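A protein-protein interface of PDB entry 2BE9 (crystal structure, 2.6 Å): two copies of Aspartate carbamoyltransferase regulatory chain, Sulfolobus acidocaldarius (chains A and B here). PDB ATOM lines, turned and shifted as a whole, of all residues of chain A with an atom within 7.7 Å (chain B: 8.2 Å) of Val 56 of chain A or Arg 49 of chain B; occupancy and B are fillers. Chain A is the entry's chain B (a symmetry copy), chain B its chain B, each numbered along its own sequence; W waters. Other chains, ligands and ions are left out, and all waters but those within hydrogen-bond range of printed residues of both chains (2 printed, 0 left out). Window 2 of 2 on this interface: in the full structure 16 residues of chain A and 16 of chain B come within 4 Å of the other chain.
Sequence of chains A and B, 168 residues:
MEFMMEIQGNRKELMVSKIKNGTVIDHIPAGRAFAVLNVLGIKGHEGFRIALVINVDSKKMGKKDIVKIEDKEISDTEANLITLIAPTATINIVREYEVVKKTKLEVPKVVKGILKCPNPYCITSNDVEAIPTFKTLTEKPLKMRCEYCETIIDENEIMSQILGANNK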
ATOM      1  N   MET A  15     -20.818 -26.651  -4.766  1.00  0.00           N
ATOM      2  CA  MET A  15     -20.691 -25.249  -5.261  1.00  0.00           C
ATOM      3  C   MET A  15     -19.227 -24.778  -5.219  1.00  0.00           C
ATOM      4  O   MET A  15     -18.880 -23.756  -5.813  1.00  0.00           O
ATOM      5  CB  MET A  15     -21.601 -24.313  -4.449  1.00  0.00           C
ATOM      6  CG  MET A  15     -21.898 -22.980  -5.130  1.00  0.00           C
ATOM      7  SD  MET A  15     -22.641 -21.744  -4.035  1.00  0.00           S
ATOM      8  CE  MET A  15     -21.947 -20.220  -4.693  1.00  0.00           C
ATOM      9  N   VAL A  16     -18.373 -25.515  -4.507  1.00  0.00           N
ATOM     10  CA  VAL A  16     -16.922 -25.277  -4.582  1.00  0.00           C
ATOM     11  C   VAL A  16     -16.204 -26.411  -5.321  1.00  0.00           C
ATOM     12  O   VAL A  16     -16.524 -27.593  -5.137  1.00  0.00           O
ATOM     13  CB  VAL A  16     -16.265 -25.007  -3.188  1.00  0.00           C
ATOM     14  CG1 VAL A  16     -16.093 -26.291  -2.378  1.00  0.00           C
ATOM     15  CG2 VAL A  16     -14.932 -24.297  -3.358  1.00  0.00           C
ATOM     16  N   ASP A  26     -17.561 -32.582   5.209  1.00  0.00           N
ATOM     17  CA  ASP A  26     -18.900 -32.443   4.632  1.00  0.00           C
ATOM     18  C   ASP A  26     -19.926 -32.650   5.739  1.00  0.00           C
ATOM     19  O   ASP A  26     -19.575 -33.068   6.845  1.00  0.00           O
ATOM     20  CB  ASP A  26     -19.090 -33.506   3.560  1.00  0.00           C
ATOM     21  CG  ASP A  26     -20.165 -33.151   2.529  1.00  0.00           C
ATOM     22  OD1 ASP A  26     -21.043 -32.292   2.753  1.00  0.00           O
ATOM     23  OD2 ASP A  26     -20.126 -33.762   1.453  1.00  0.00           O
ATOM     24  N   ILE A  28     -21.649 -30.694   7.736  1.00  0.00           N
ATOM     25  CA  ILE A  28     -21.656 -29.839   8.902  1.00  0.00           C
ATOM     26  C   ILE A  28     -23.036 -29.209   8.966  1.00  0.00           C
ATOM     27  O   ILE A  28     -23.554 -28.786   7.930  1.00  0.00           O
ATOM     28  CB  ILE A  28     -20.610 -28.731   8.747  1.00  0.00           C
ATOM     29  CG1 ILE A  28     -19.219 -29.349   8.572  1.00  0.00           C
ATOM     30  CG2 ILE A  28     -20.643 -27.786   9.941  1.00  0.00           C
ATOM     31  CD1 ILE A  28     -18.235 -28.453   7.862  1.00  0.00           C
ATOM     32  N   ALA A  30     -25.734 -26.482   8.957  1.00  0.00           N
ATOM     33  CA  ALA A  30     -25.798 -25.127   8.404  1.00  0.00           C
ATOM     34  C   ALA A  30     -25.328 -24.076   9.403  1.00  0.00           C
ATOM     35  O   ALA A  30     -25.746 -24.078  10.559  1.00  0.00           O
ATOM     36  CB  ALA A  30     -27.209 -24.815   7.948  1.00  0.00           C
ATOM     37  N   GLY A  31     -24.438 -23.196   8.960  1.00  0.00           N
ATOM     38  CA  GLY A  31     -23.963 -22.095   9.803  1.00  0.00           C
ATOM     39  C   GLY A  31     -22.779 -22.424  10.702  1.00  0.00           C
ATOM     40  O   GLY A  31     -22.182 -21.526  11.288  1.00  0.00           O
ATOM     41  N   LEU A  52     -14.878 -22.651   2.132  1.00  0.00           N
ATOM     42  CA  LEU A  52     -16.124 -22.977   2.781  1.00  0.00           C
ATOM     43  C   LEU A  52     -17.304 -22.604   1.895  1.00  0.00           C
ATOM     44  O   LEU A  52     -17.270 -21.609   1.171  1.00  0.00           O
ATOM     45  CB  LEU A  52     -16.300 -22.260   4.108  1.00  0.00           C
ATOM     46  CG  LEU A  52     -15.338 -21.386   4.888  1.00  0.00           C
ATOM     47  CD1 LEU A  52     -15.897 -21.364   6.276  1.00  0.00           C
ATOM     48  CD2 LEU A  52     -13.951 -21.893   4.942  1.00  0.00           C
ATOM     49  N   VAL A  53     -18.349 -23.423   1.962  1.00  0.00           N
ATOM     50  CA  VAL A  53     -19.649 -23.011   1.486  1.00  0.00           C
ATOM     51  C   VAL A  53     -20.601 -23.115   2.667  1.00  0.00           C
ATOM     52  O   VAL A  53     -20.546 -24.062   3.443  1.00  0.00           O
ATOM     53  CB  VAL A  53     -20.110 -23.805   0.244  1.00  0.00           C
ATOM     54  CG1 VAL A  53     -19.056 -23.705  -0.833  1.00  0.00           C
ATOM     55  CG2 VAL A  53     -20.342 -25.261   0.573  1.00  0.00           C
ATOM     56  N   ILE A  54     -21.462 -22.123   2.819  1.00  0.00           N
ATOM     57  CA  ILE A  54     -22.328 -22.075   3.974  1.00  0.00           C
ATOM     58  C   ILE A  54     -23.786 -21.988   3.551  1.00  0.00           C
ATOM     59  O   ILE A  54     -24.132 -21.226   2.648  1.00  0.00           O
ATOM     60  CB  ILE A  54     -21.878 -20.932   4.913  1.00  0.00           C
ATOM     61  CG1 ILE A  54     -20.606 -21.386   5.637  1.00  0.00           C
ATOM     62  CG2 ILE A  54     -22.934 -20.587   5.948  1.00  0.00           C
ATOM     63  CD1 ILE A  54     -19.617 -20.317   5.811  1.00  0.00           C
ATOM     64  N   ASN A  55     -24.625 -22.802   4.196  1.00  0.00           N
ATOM     65  CA  ASN A  55     -26.064 -22.830   3.960  1.00  0.00           C
ATOM     66  C   ASN A  55     -26.471 -23.445   2.627  1.00  0.00           C
ATOM     67  O   ASN A  55     -27.544 -23.152   2.102  1.00  0.00           O
ATOM     68  CB  ASN A  55     -26.678 -21.438   4.112  1.00  0.00           C
ATOM     69  CG  ASN A  55     -26.755 -20.997   5.553  1.00  0.00           C
ATOM     70  OD1 ASN A  55     -26.300 -19.903   5.908  1.00  0.00           O
ATOM     71  ND2 ASN A  55     -27.329 -21.851   6.402  1.00  0.00           N
ATOM     72  N   VAL A  56     -25.626 -24.313   2.086  1.00  0.00           N
ATOM     73  CA  VAL A  56     -25.968 -24.992   0.842  1.00  0.00           C
ATOM     74  C   VAL A  56     -26.944 -26.134   1.094  1.00  0.00           C
ATOM     75  O   VAL A  56     -27.102 -26.593   2.241  1.00  0.00           O
ATOM     76  CB  VAL A  56     -24.721 -25.496   0.083  1.00  0.00           C
ATOM     77  CG1 VAL A  56     -23.826 -24.319  -0.269  1.00  0.00           C
ATOM     78  CG2 VAL A  56     -23.965 -26.529   0.900  1.00  0.00           C
ATOM     79  N   ASP A  57     -27.601 -26.565   0.012  1.00  0.00           N
ATOM     80  CA  ASP A  57     -28.601 -27.636   0.046  1.00  0.00           C
ATOM     81  C   ASP A  57     -27.987 -28.950   0.463  1.00  0.00           C
ATOM     82  O   ASP A  57     -26.831 -29.248   0.159  1.00  0.00           O
ATOM     83  CB  ASP A  57     -29.247 -27.829  -1.324  1.00  0.00           C
ATOM     84  CG  ASP A  57     -30.218 -26.714  -1.690  1.00  0.00           C
ATOM     85  OD1 ASP A  57     -30.723 -25.987  -0.793  1.00  0.00           O
ATOM     86  OD2 ASP A  57     -30.485 -26.586  -2.904  1.00  0.00           O
ATOM     87  N   SER A  58     -28.782 -29.728   1.174  1.00  0.00           N
ATOM     88  CA  SER A  58     -28.390 -31.048   1.600  1.00  0.00           C
ATOM     89  C   SER A  58     -29.649 -31.861   1.513  1.00  0.00           C
ATOM     90  O   SER A  58     -30.660 -31.489   2.108  1.00  0.00           O
ATOM     91  CB  SER A  58     -27.907 -31.029   3.044  1.00  0.00           C
ATOM     92  OG  SER A  58     -27.636 -32.344   3.492  1.00  0.00           O
ATOM     93  N   LYS A  59     -29.595 -32.959   0.763  1.00  0.00           N
ATOM     94  CA  LYS A  59     -30.751 -33.824   0.630  1.00  0.00           C
ATOM     95  C   LYS A  59     -31.169 -34.463   1.961  1.00  0.00           C
ATOM     96  O   LYS A  59     -32.360 -34.543   2.270  1.00  0.00           O
ATOM     97  CB  LYS A  59     -30.524 -34.877  -0.457  1.00  0.00           C
ATOM     98  CG  LYS A  59     -31.317 -34.606  -1.718  1.00  0.00           C
ATOM     99  CD  LYS A  59     -30.468 -34.127  -2.875  1.00  0.00           C
ATOM    100  CE  LYS A  59     -31.371 -33.661  -4.022  1.00  0.00           C
ATOM    101  NZ  LYS A  59     -30.897 -34.124  -5.353  1.00  0.00           N
ATOM    102  N   MET A  61     -30.105 -33.451   5.176  1.00  0.00           N
ATOM    103  CA  MET A  61     -30.102 -32.540   6.336  1.00  0.00           C
ATOM    104  C   MET A  61     -30.908 -31.258   6.145  1.00  0.00           C
ATOM    105  O   MET A  61     -31.053 -30.488   7.095  1.00  0.00           O
ATOM    106  CB  MET A  61     -28.672 -32.134   6.700  1.00  0.00           C
ATOM    107  CG  MET A  61     -27.729 -33.261   7.045  1.00  0.00           C
ATOM    108  SD  MET A  61     -26.018 -32.672   7.128  1.00  0.00           S
ATOM    109  CE  MET A  61     -26.097 -31.565   8.556  1.00  0.00           C
ATOM    110  N   GLY A  62     -31.409 -31.026   4.924  1.00  0.00           N
ATOM    111  CA  GLY A  62     -32.037 -29.753   4.551  1.00  0.00           C
ATOM    112  C   GLY A  62     -30.980 -28.749   4.106  1.00  0.00           C
ATOM    113  O   GLY A  62     -30.823 -28.469   2.914  1.00  0.00           O
ATOM    114  N   LYS A  63     -30.249 -28.199   5.071  1.00  0.00           N
ATOM    115  CA  LYS A  63     -29.098 -27.353   4.764  1.00  0.00           C
ATOM    116  C   LYS A  63     -27.827 -27.922   5.391  1.00  0.00           C
ATOM    117  O   LYS A  63     -27.882 -28.666   6.376  1.00  0.00           O
ATOM    118  CB  LYS A  63     -29.311 -25.903   5.241  1.00  0.00           C
ATOM    119  CG  LYS A  63     -30.582 -25.209   4.759  1.00  0.00           C
ATOM    120  CD  LYS A  63     -30.565 -24.905   3.276  1.00  0.00           C
ATOM    121  CE  LYS A  63     -31.810 -24.123   2.856  1.00  0.00           C
ATOM    122  NZ  LYS A  63     -31.777 -23.863   1.390  1.00  0.00           N
ATOM    123  N   LYS A  64     -26.684 -27.562   4.819  1.00  0.00           N
ATOM    124  CA  LYS A  64     -25.401 -27.929   5.381  1.00  0.00           C
ATOM    125  C   LYS A  64     -24.291 -26.902   5.068  1.00  0.00           C
ATOM    126  O   LYS A  64     -24.529 -25.901   4.375  1.00  0.00           O
ATOM    127  CB  LYS A  64     -25.020 -29.363   4.965  1.00  0.00           C
ATOM    128  CG  LYS A  64     -24.059 -29.506   3.768  1.00  0.00           C
ATOM    129  CD  LYS A  64     -24.718 -30.036   2.543  1.00  0.00           C
ATOM    130  CE  LYS A  64     -23.696 -30.438   1.485  1.00  0.00           C
ATOM    131  NZ  LYS A  64     -23.362 -31.878   1.477  1.00  0.00           N
ATOM    132  N   ASP A  65     -23.101 -27.145   5.626  1.00  0.00           N
ATOM    133  CA  ASP A  65     -21.891 -26.397   5.336  1.00  0.00           C
ATOM    134  C   ASP A  65     -20.859 -27.433   4.914  1.00  0.00           C
ATOM    135  O   ASP A  65     -20.902 -28.582   5.365  1.00  0.00           O
ATOM    136  CB  ASP A  65     -21.349 -25.697   6.583  1.00  0.00           C
ATOM    137  CG  ASP A  65     -22.180 -24.477   7.039  1.00  0.00           C
ATOM    138  OD1 ASP A  65     -21.676 -23.792   7.952  1.00  0.00           O
ATOM    139  OD2 ASP A  65     -23.295 -24.179   6.545  1.00  0.00           O
ATOM    140  N   ILE A  66     -19.926 -27.021   4.058  1.00  0.00           N
ATOM    141  CA  ILE A  66     -18.799 -27.842   3.700  1.00  0.00           C
ATOM    142  C   ILE A  66     -17.509 -27.056   3.897  1.00  0.00           C
ATOM    143  O   ILE A  66     -17.411 -25.879   3.504  1.00  0.00           O
ATOM    144  CB  ILE A  66     -18.851 -28.288   2.231  1.00  0.00           C
ATOM    145  CG1 ILE A  66     -20.167 -29.001   1.895  1.00  0.00           C
ATOM    146  CG2 ILE A  66     -17.650 -29.179   1.893  1.00  0.00           C
ATOM    147  CD1 ILE A  66     -20.477 -29.011   0.375  1.00  0.00           C
ATOM    148  N   ILE B  19     -21.830 -17.607  -9.296  1.00  0.00           N
ATOM    149  CA  ILE B  19     -23.008 -17.346  -8.492  1.00  0.00           C
ATOM    150  C   ILE B  19     -24.144 -16.861  -9.400  1.00  0.00           C
ATOM    151  O   ILE B  19     -23.915 -16.082 -10.325  1.00  0.00           O
ATOM    152  CB  ILE B  19     -22.661 -16.342  -7.332  1.00  0.00           C
ATOM    153  CG1 ILE B  19     -23.765 -16.269  -6.286  1.00  0.00           C
ATOM    154  CG2 ILE B  19     -22.302 -14.931  -7.843  1.00  0.00           C
ATOM    155  CD1 ILE B  19     -23.631 -15.037  -5.381  1.00  0.00           C
ATOM    156  N   LYS B  20     -25.361 -17.351  -9.164  1.00  0.00           N
ATOM    157  CA  LYS B  20     -26.494 -16.952  -9.993  1.00  0.00           C
ATOM    158  C   LYS B  20     -26.865 -15.505  -9.708  1.00  0.00           C
ATOM    159  O   LYS B  20     -26.927 -14.685 -10.635  1.00  0.00           O
ATOM    160  CB  LYS B  20     -27.697 -17.887  -9.810  1.00  0.00           C
ATOM    161  CG  LYS B  20     -28.813 -17.683 -10.852  1.00  0.00           C
ATOM    162  CD  LYS B  20     -30.051 -18.549 -10.570  1.00  0.00           C
ATOM    163  CE  LYS B  20     -31.325 -17.864 -11.073  1.00  0.00           C
ATOM    164  NZ  LYS B  20     -32.530 -18.210 -10.263  1.00  0.00           N
ATOM    165  N   ASN B  21     -27.090 -15.189  -8.429  1.00  0.00           N
ATOM    166  CA  ASN B  21     -27.417 -13.819  -8.015  1.00  0.00           C
ATOM    167  C   ASN B  21     -26.776 -13.426  -6.694  1.00  0.00           C
ATOM    168  O   ASN B  21     -26.889 -14.163  -5.714  1.00  0.00           O
ATOM    169  CB  ASN B  21     -28.927 -13.638  -7.921  1.00  0.00           C
ATOM    170  CG  ASN B  21     -29.635 -14.030  -9.195  1.00  0.00           C
ATOM    171  OD1 ASN B  21     -29.523 -13.347 -10.216  1.00  0.00           O
ATOM    172  ND2 ASN B  21     -30.353 -15.150  -9.154  1.00  0.00           N
ATOM    173  N   GLY B  22     -26.109 -12.271  -6.664  1.00  0.00           N
ATOM    174  CA  GLY B  22     -25.589 -11.719  -5.411  1.00  0.00           C
ATOM    175  C   GLY B  22     -24.363 -10.824  -5.510  1.00  0.00           C
ATOM    176  O   GLY B  22     -24.232 -10.038  -6.455  1.00  0.00           O
ATOM    177  N   THR B  23     -23.468 -10.942  -4.525  1.00  0.00           N
ATOM    178  CA  THR B  23     -22.275 -10.089  -4.443  1.00  0.00           C
ATOM    179  C   THR B  23     -21.009 -10.919  -4.400  1.00  0.00           C
ATOM    180  O   THR B  23     -20.928 -11.913  -3.680  1.00  0.00           O
ATOM    181  CB  THR B  23     -22.289  -9.183  -3.192  1.00  0.00           C
ATOM    182  OG1 THR B  23     -23.517  -8.452  -3.143  1.00  0.00           O
ATOM    183  CG2 THR B  23     -21.120  -8.205  -3.218  1.00  0.00           C
ATOM    184  N   ILE B  42     -22.140 -10.217   8.683  1.00  0.00           N
ATOM    185  CA  ILE B  42     -22.600 -11.509   8.172  1.00  0.00           C
ATOM    186  C   ILE B  42     -21.888 -12.671   8.870  1.00  0.00           C
ATOM    187  O   ILE B  42     -20.688 -12.896   8.644  1.00  0.00           O
ATOM    188  CB  ILE B  42     -22.351 -11.624   6.659  1.00  0.00           C
ATOM    189  CG1 ILE B  42     -23.151 -10.570   5.901  1.00  0.00           C
ATOM    190  CG2 ILE B  42     -22.708 -13.026   6.166  1.00  0.00           C
ATOM    191  CD1 ILE B  42     -22.585 -10.243   4.530  1.00  0.00           C
ATOM    192  N   GLU B  46     -27.245 -14.734   8.069  1.00  0.00           N
ATOM    193  CA  GLU B  46     -27.848 -16.079   8.122  1.00  0.00           C
ATOM    194  C   GLU B  46     -29.068 -16.290   7.227  1.00  0.00           C
ATOM    195  O   GLU B  46     -29.862 -15.374   7.003  1.00  0.00           O
ATOM    196  CB  GLU B  46     -28.161 -16.498   9.546  1.00  0.00           C
ATOM    197  CG  GLU B  46     -26.958 -17.107  10.207  1.00  0.00           C
ATOM    198  CD  GLU B  46     -27.058 -17.060  11.707  1.00  0.00           C
ATOM    199  OE1 GLU B  46     -26.012 -17.203  12.378  1.00  0.00           O
ATOM    200  OE2 GLU B  46     -28.183 -16.869  12.218  1.00  0.00           O
ATOM    201  N   GLY B  47     -29.183 -17.522   6.723  1.00  0.00           N
ATOM    202  CA  GLY B  47     -30.188 -17.897   5.734  1.00  0.00           C
ATOM    203  C   GLY B  47     -29.520 -18.162   4.392  1.00  0.00           C
ATOM    204  O   GLY B  47     -29.535 -19.295   3.888  1.00  0.00           O
ATOM    205  N   PHE B  48     -28.915 -17.110   3.837  1.00  0.00           N
ATOM    206  CA  PHE B  48     -28.337 -17.104   2.482  1.00  0.00           C
ATOM    207  C   PHE B  48     -26.965 -17.776   2.362  1.00  0.00           C
ATOM    208  O   PHE B  48     -26.130 -17.721   3.272  1.00  0.00           O
ATOM    209  CB  PHE B  48     -28.272 -15.664   1.927  1.00  0.00           C
ATOM    210  CG  PHE B  48     -27.763 -14.635   2.931  1.00  0.00           C
ATOM    211  CD1 PHE B  48     -26.394 -14.541   3.236  1.00  0.00           C
ATOM    212  CD2 PHE B  48     -28.656 -13.757   3.565  1.00  0.00           C
ATOM    213  CE1 PHE B  48     -25.922 -13.594   4.173  1.00  0.00           C
ATOM    214  CE2 PHE B  48     -28.203 -12.806   4.497  1.00  0.00           C
ATOM    215  CZ  PHE B  48     -26.829 -12.725   4.807  1.00  0.00           C
ATOM    216  N   ARG B  49     -26.748 -18.393   1.205  1.00  0.00           N
ATOM    217  CA  ARG B  49     -25.506 -19.073   0.883  1.00  0.00           C
ATOM    218  C   ARG B  49     -24.326 -18.119   0.930  1.00  0.00           C
ATOM    219  O   ARG B  49     -24.436 -16.978   0.492  1.00  0.00           O
ATOM    220  CB  ARG B  49     -25.590 -19.696  -0.516  1.00  0.00           C
ATOM    221  CG  ARG B  49     -26.131 -21.117  -0.562  1.00  0.00           C
ATOM    222  CD  ARG B  49     -27.636 -21.138  -0.658  1.00  0.00           C
ATOM    223  NE  ARG B  49     -28.084 -20.721  -1.988  1.00  0.00           N
ATOM    224  CZ  ARG B  49     -28.689 -21.514  -2.869  1.00  0.00           C
ATOM    225  NH1 ARG B  49     -29.043 -21.025  -4.051  1.00  0.00           N
ATOM    226  NH2 ARG B  49     -28.945 -22.788  -2.572  1.00  0.00           N
ATOM    227  N   ILE B  50     -23.205 -18.597   1.467  1.00  0.00           N
ATOM    228  CA  ILE B  50     -21.943 -17.872   1.414  1.00  0.00           C
ATOM    229  C   ILE B  50     -20.828 -18.819   1.000  1.00  0.00           C
ATOM    230  O   ILE B  50     -20.782 -19.965   1.426  1.00  0.00           O
ATOM    231  CB  ILE B  50     -21.584 -17.223   2.780  1.00  0.00           C
ATOM    232  CG1 ILE B  50     -22.627 -16.186   3.206  1.00  0.00           C
ATOM    233  CG2 ILE B  50     -20.206 -16.558   2.739  1.00  0.00           C
ATOM    234  CD1 ILE B  50     -22.693 -16.013   4.713  1.00  0.00           C
ATOM    235  N   ALA B  51     -19.933 -18.336   0.151  1.00  0.00           N
ATOM    236  CA  ALA B  51     -18.725 -19.069  -0.167  1.00  0.00           C
ATOM    237  C   ALA B  51     -17.501 -18.198   0.088  1.00  0.00           C
ATOM    238  O   ALA B  51     -17.510 -16.997  -0.219  1.00  0.00           O
ATOM    239  CB  ALA B  51     -18.740 -19.543  -1.590  1.00  0.00           C
ATOM    240  N   LEU B  52     -16.468 -18.800   0.686  1.00  0.00           N
ATOM    241  CA  LEU B  52     -15.164 -18.184   0.744  1.00  0.00           C
ATOM    242  C   LEU B  52     -14.097 -19.134   0.218  1.00  0.00           C
ATOM    243  O   LEU B  52     -14.175 -20.349   0.407  1.00  0.00           O
ATOM    244  CB  LEU B  52     -14.767 -17.783   2.154  1.00  0.00           C
ATOM    245  CG  LEU B  52     -15.563 -17.810   3.445  1.00  0.00           C
ATOM    246  CD1 LEU B  52     -14.818 -16.891   4.361  1.00  0.00           C
ATOM    247  CD2 LEU B  52     -16.956 -17.332   3.320  1.00  0.00           C
ATOM    248  N   VAL B  67     -14.808 -13.631  -1.404  1.00  0.00           N
ATOM    249  CA  VAL B  67     -16.071 -13.892  -0.737  1.00  0.00           C
ATOM    250  C   VAL B  67     -17.234 -13.799  -1.745  1.00  0.00           C
ATOM    251  O   VAL B  67     -17.254 -12.939  -2.632  1.00  0.00           O
ATOM    252  CB  VAL B  67     -16.301 -12.930   0.460  1.00  0.00           C
ATOM    253  CG1 VAL B  67     -17.599 -13.267   1.172  1.00  0.00           C
ATOM    254  CG2 VAL B  67     -15.149 -13.002   1.434  1.00  0.00           C
ATOM    255  N   LYS B  68     -18.192 -14.702  -1.603  1.00  0.00           N
ATOM    256  CA  LYS B  68     -19.359 -14.715  -2.444  1.00  0.00           C
ATOM    257  C   LYS B  68     -20.591 -14.883  -1.575  1.00  0.00           C
ATOM    258  O   LYS B  68     -20.707 -15.857  -0.826  1.00  0.00           O
ATOM    259  CB  LYS B  68     -19.245 -15.831  -3.483  1.00  0.00           C
ATOM    260  CG  LYS B  68     -18.301 -15.481  -4.628  1.00  0.00           C
ATOM    261  CD  LYS B  68     -18.116 -16.647  -5.557  1.00  0.00           C
ATOM    262  CE  LYS B  68     -17.101 -16.317  -6.633  1.00  0.00           C
ATOM    263  NZ  LYS B  68     -17.204 -17.249  -7.816  1.00  0.00           N
ATOM    264  N   ILE B  69     -21.494 -13.909  -1.659  1.00  0.00           N
ATOM    265  CA  ILE B  69     -22.724 -13.931  -0.894  1.00  0.00           C
ATOM    266  C   ILE B  69     -23.869 -14.011  -1.872  1.00  0.00           C
ATOM    267  O   ILE B  69     -24.090 -13.071  -2.641  1.00  0.00           O
ATOM    268  CB  ILE B  69     -22.865 -12.661  -0.028  1.00  0.00           C
ATOM    269  CG1 ILE B  69     -21.647 -12.508   0.898  1.00  0.00           C
ATOM    270  CG2 ILE B  69     -24.179 -12.698   0.797  1.00  0.00           C
ATOM    271  CD1 ILE B  69     -21.139 -11.108   1.021  1.00  0.00           C
ATOM    272  N   GLU B  70     -24.577 -15.139  -1.873  1.00  0.00           N
ATOM    273  CA  GLU B  70     -25.787 -15.260  -2.690  1.00  0.00           C
ATOM    274  C   GLU B  70     -26.891 -14.366  -2.180  1.00  0.00           C
ATOM    275  O   GLU B  70     -26.977 -14.097  -0.980  1.00  0.00           O
ATOM    276  CB  GLU B  70     -26.316 -16.690  -2.767  1.00  0.00           C
ATOM    277  CG  GLU B  70     -25.542 -17.604  -3.683  1.00  0.00           C
ATOM    278  CD  GLU B  70     -26.439 -18.359  -4.635  1.00  0.00           C
ATOM    279  OE1 GLU B  70     -26.833 -17.787  -5.685  1.00  0.00           O
ATOM    280  OE2 GLU B  70     -26.745 -19.532  -4.340  1.00  0.00           O
ATOM    281  N   ASP B  71     -27.707 -13.897  -3.124  1.00  0.00           N
ATOM    282  CA  ASP B  71     -29.010 -13.295  -2.857  1.00  0.00           C
ATOM    283  C   ASP B  71     -28.982 -12.025  -2.035  1.00  0.00           C
ATOM    284  O   ASP B  71     -29.996 -11.614  -1.481  1.00  0.00           O
ATOM    285  CB  ASP B  71     -29.955 -14.320  -2.220  1.00  0.00           C
ATOM    286  CG  ASP B  71     -30.240 -15.490  -3.135  1.00  0.00           C
ATOM    287  OD1 ASP B  71     -30.341 -16.614  -2.634  1.00  0.00           O
ATOM    288  OD2 ASP B  71     -30.358 -15.295  -4.359  1.00  0.00           O
ATOM    289  N   LYS B  72     -27.814 -11.403  -1.966  1.00  0.00           N
ATOM    290  CA  LYS B  72     -27.658 -10.142  -1.274  1.00  0.00           C
ATOM    291  C   LYS B  72     -26.790  -9.229  -2.128  1.00  0.00           C
ATOM    292  O   LYS B  72     -25.712  -9.621  -2.596  1.00  0.00           O
ATOM    293  CB  LYS B  72     -27.078 -10.358   0.129  1.00  0.00           C
ATOM    294  CG  LYS B  72     -26.955  -9.102   0.991  1.00  0.00           C
ATOM    295  CD  LYS B  72     -27.641  -9.314   2.362  1.00  0.00           C
ATOM    296  CE  LYS B  72     -27.649  -8.040   3.266  1.00  0.00           C
ATOM    297  NZ  LYS B  72     -26.583  -8.079   4.316  1.00  0.00           N
HETATM  298  O   HOH W   1     -26.807 -16.680   5.525  1.00  0.00           O
HETATM  299  O   HOH W   2     -27.236 -25.038  -2.327  1.00  0.00           O
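O of Leu 52 of chain A touches O of Ile 50 of chain B, at 3.9 Å. Leu 52 of chain A touches Ala 51 of chain B. Val 53 of chain A touches Ile 50 of chain B (CA to O, 3.3 Å). O of Ile 54 of chain A touches CA of Arg 49 of chain B, at 3.1 Å. Gly 47 of chain B touches Asn 55 of chain A. Asn 55 of chain A touches Arg 49 of chain B (O to CD, 3.4 Å). CG of Arg 49 of chain B touches CG1 of Val 56 of chain A, 3.96 Å away.
OE2 of Glu 70 of chain B is in salt-bridge range of NH1 of Arg 49 of chain B (2.8 Å). N of Lys 68 of chain B lies within hydrogen-bond range of O of Ala 51 of chain B. N of Val 53 of chain A lies within hydrogen-bond range of O of Ile 66 of chain A, 3.0 Å away. O of Lys 64 of chain A sits at hydrogen-bond distance from N of Asn 55 of chain A, 3.1 Å away. OD2 of Asp 65 of chain A lies within hydrogen-bond range of N of Asn 55 of chain A. N of Lys 64 of chain A is in hydrogen-bond range of O of Val 56 of chain A, 2.8 Å away.
Water W1 lies within hydrogen-bond range of O of Phe 48 of chain B (2.6 Å), N of Gly 47 of chain B (2.8 Å), N of Glu 46 of chain B (3.2 Å) and OD1 of Asn 55 of chain A (3.3 Å). Water W2 lies within hydrogen-bond range of N of Asp 57 of chain A (2.8 Å) and NH2 of Arg 49 of chain B (2.8 Å).
Hydrophobic or aromatic side chains of chain A that line the printed part of chain B: Leu 52, Ile 54 and Val 56. Among the printed residues, no Asp or Glu carboxylate lies within 4 Å of a Lys or Arg side-chain nitrogen of the other chain.
Leu 52 of chain B touches its own counterpart, Leu 52 of chain A. 1 position is printed for both chains. Of the 10 pairs that touch across the chains among the printed residues, 1 has its exchanged pair printed and touching as well.
The backbone carbonyl oxygen (O) of Phe 48 of chain B lies close to the side-chain amide oxygen (OD1) of Asn 55 of chain A, 3.4 Å away. The backbone carbonyl oxygen of Ile 50 of chain B sits at hydrogen-bond distance from the backbone NH of Ile 54 of chain A (2.7 Å). The backbone carbonyl oxygen of Leu 52 of chain B sits at hydrogen-bond distance from the backbone NH of Leu 52 of chain A (3.0 Å).
Of chain B, only Arg 49 comes within 4 Å of Val 56 of chain A. Of the printed residues of chain A, Arg 49 of chain B touches Ile 54 (3.1 Å), Asn 55 (3.4 Å) and Val 56 (3.96 Å). Of the printed residues of chain A, Leu 52 of chain B touches Leu 52. Of the printed residues of chain A, Phe 48 of chain B touches Asn 55. Of the printed residues of chain B, Leu 52 of chain A touches Ile 50, Ala 51 and Leu 52. Printed residues of chain B within 4 Å of Ile 54 of chain A: Arg 49 and Ile 50. The nearest residue of chain B that does not touch Val 56 of chain A is Ile 50 of chain B (5.6 Å). The nearest residue of chain A that does not touch Arg 49 of chain B is Asp 57 of chain A (4.1 Å).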
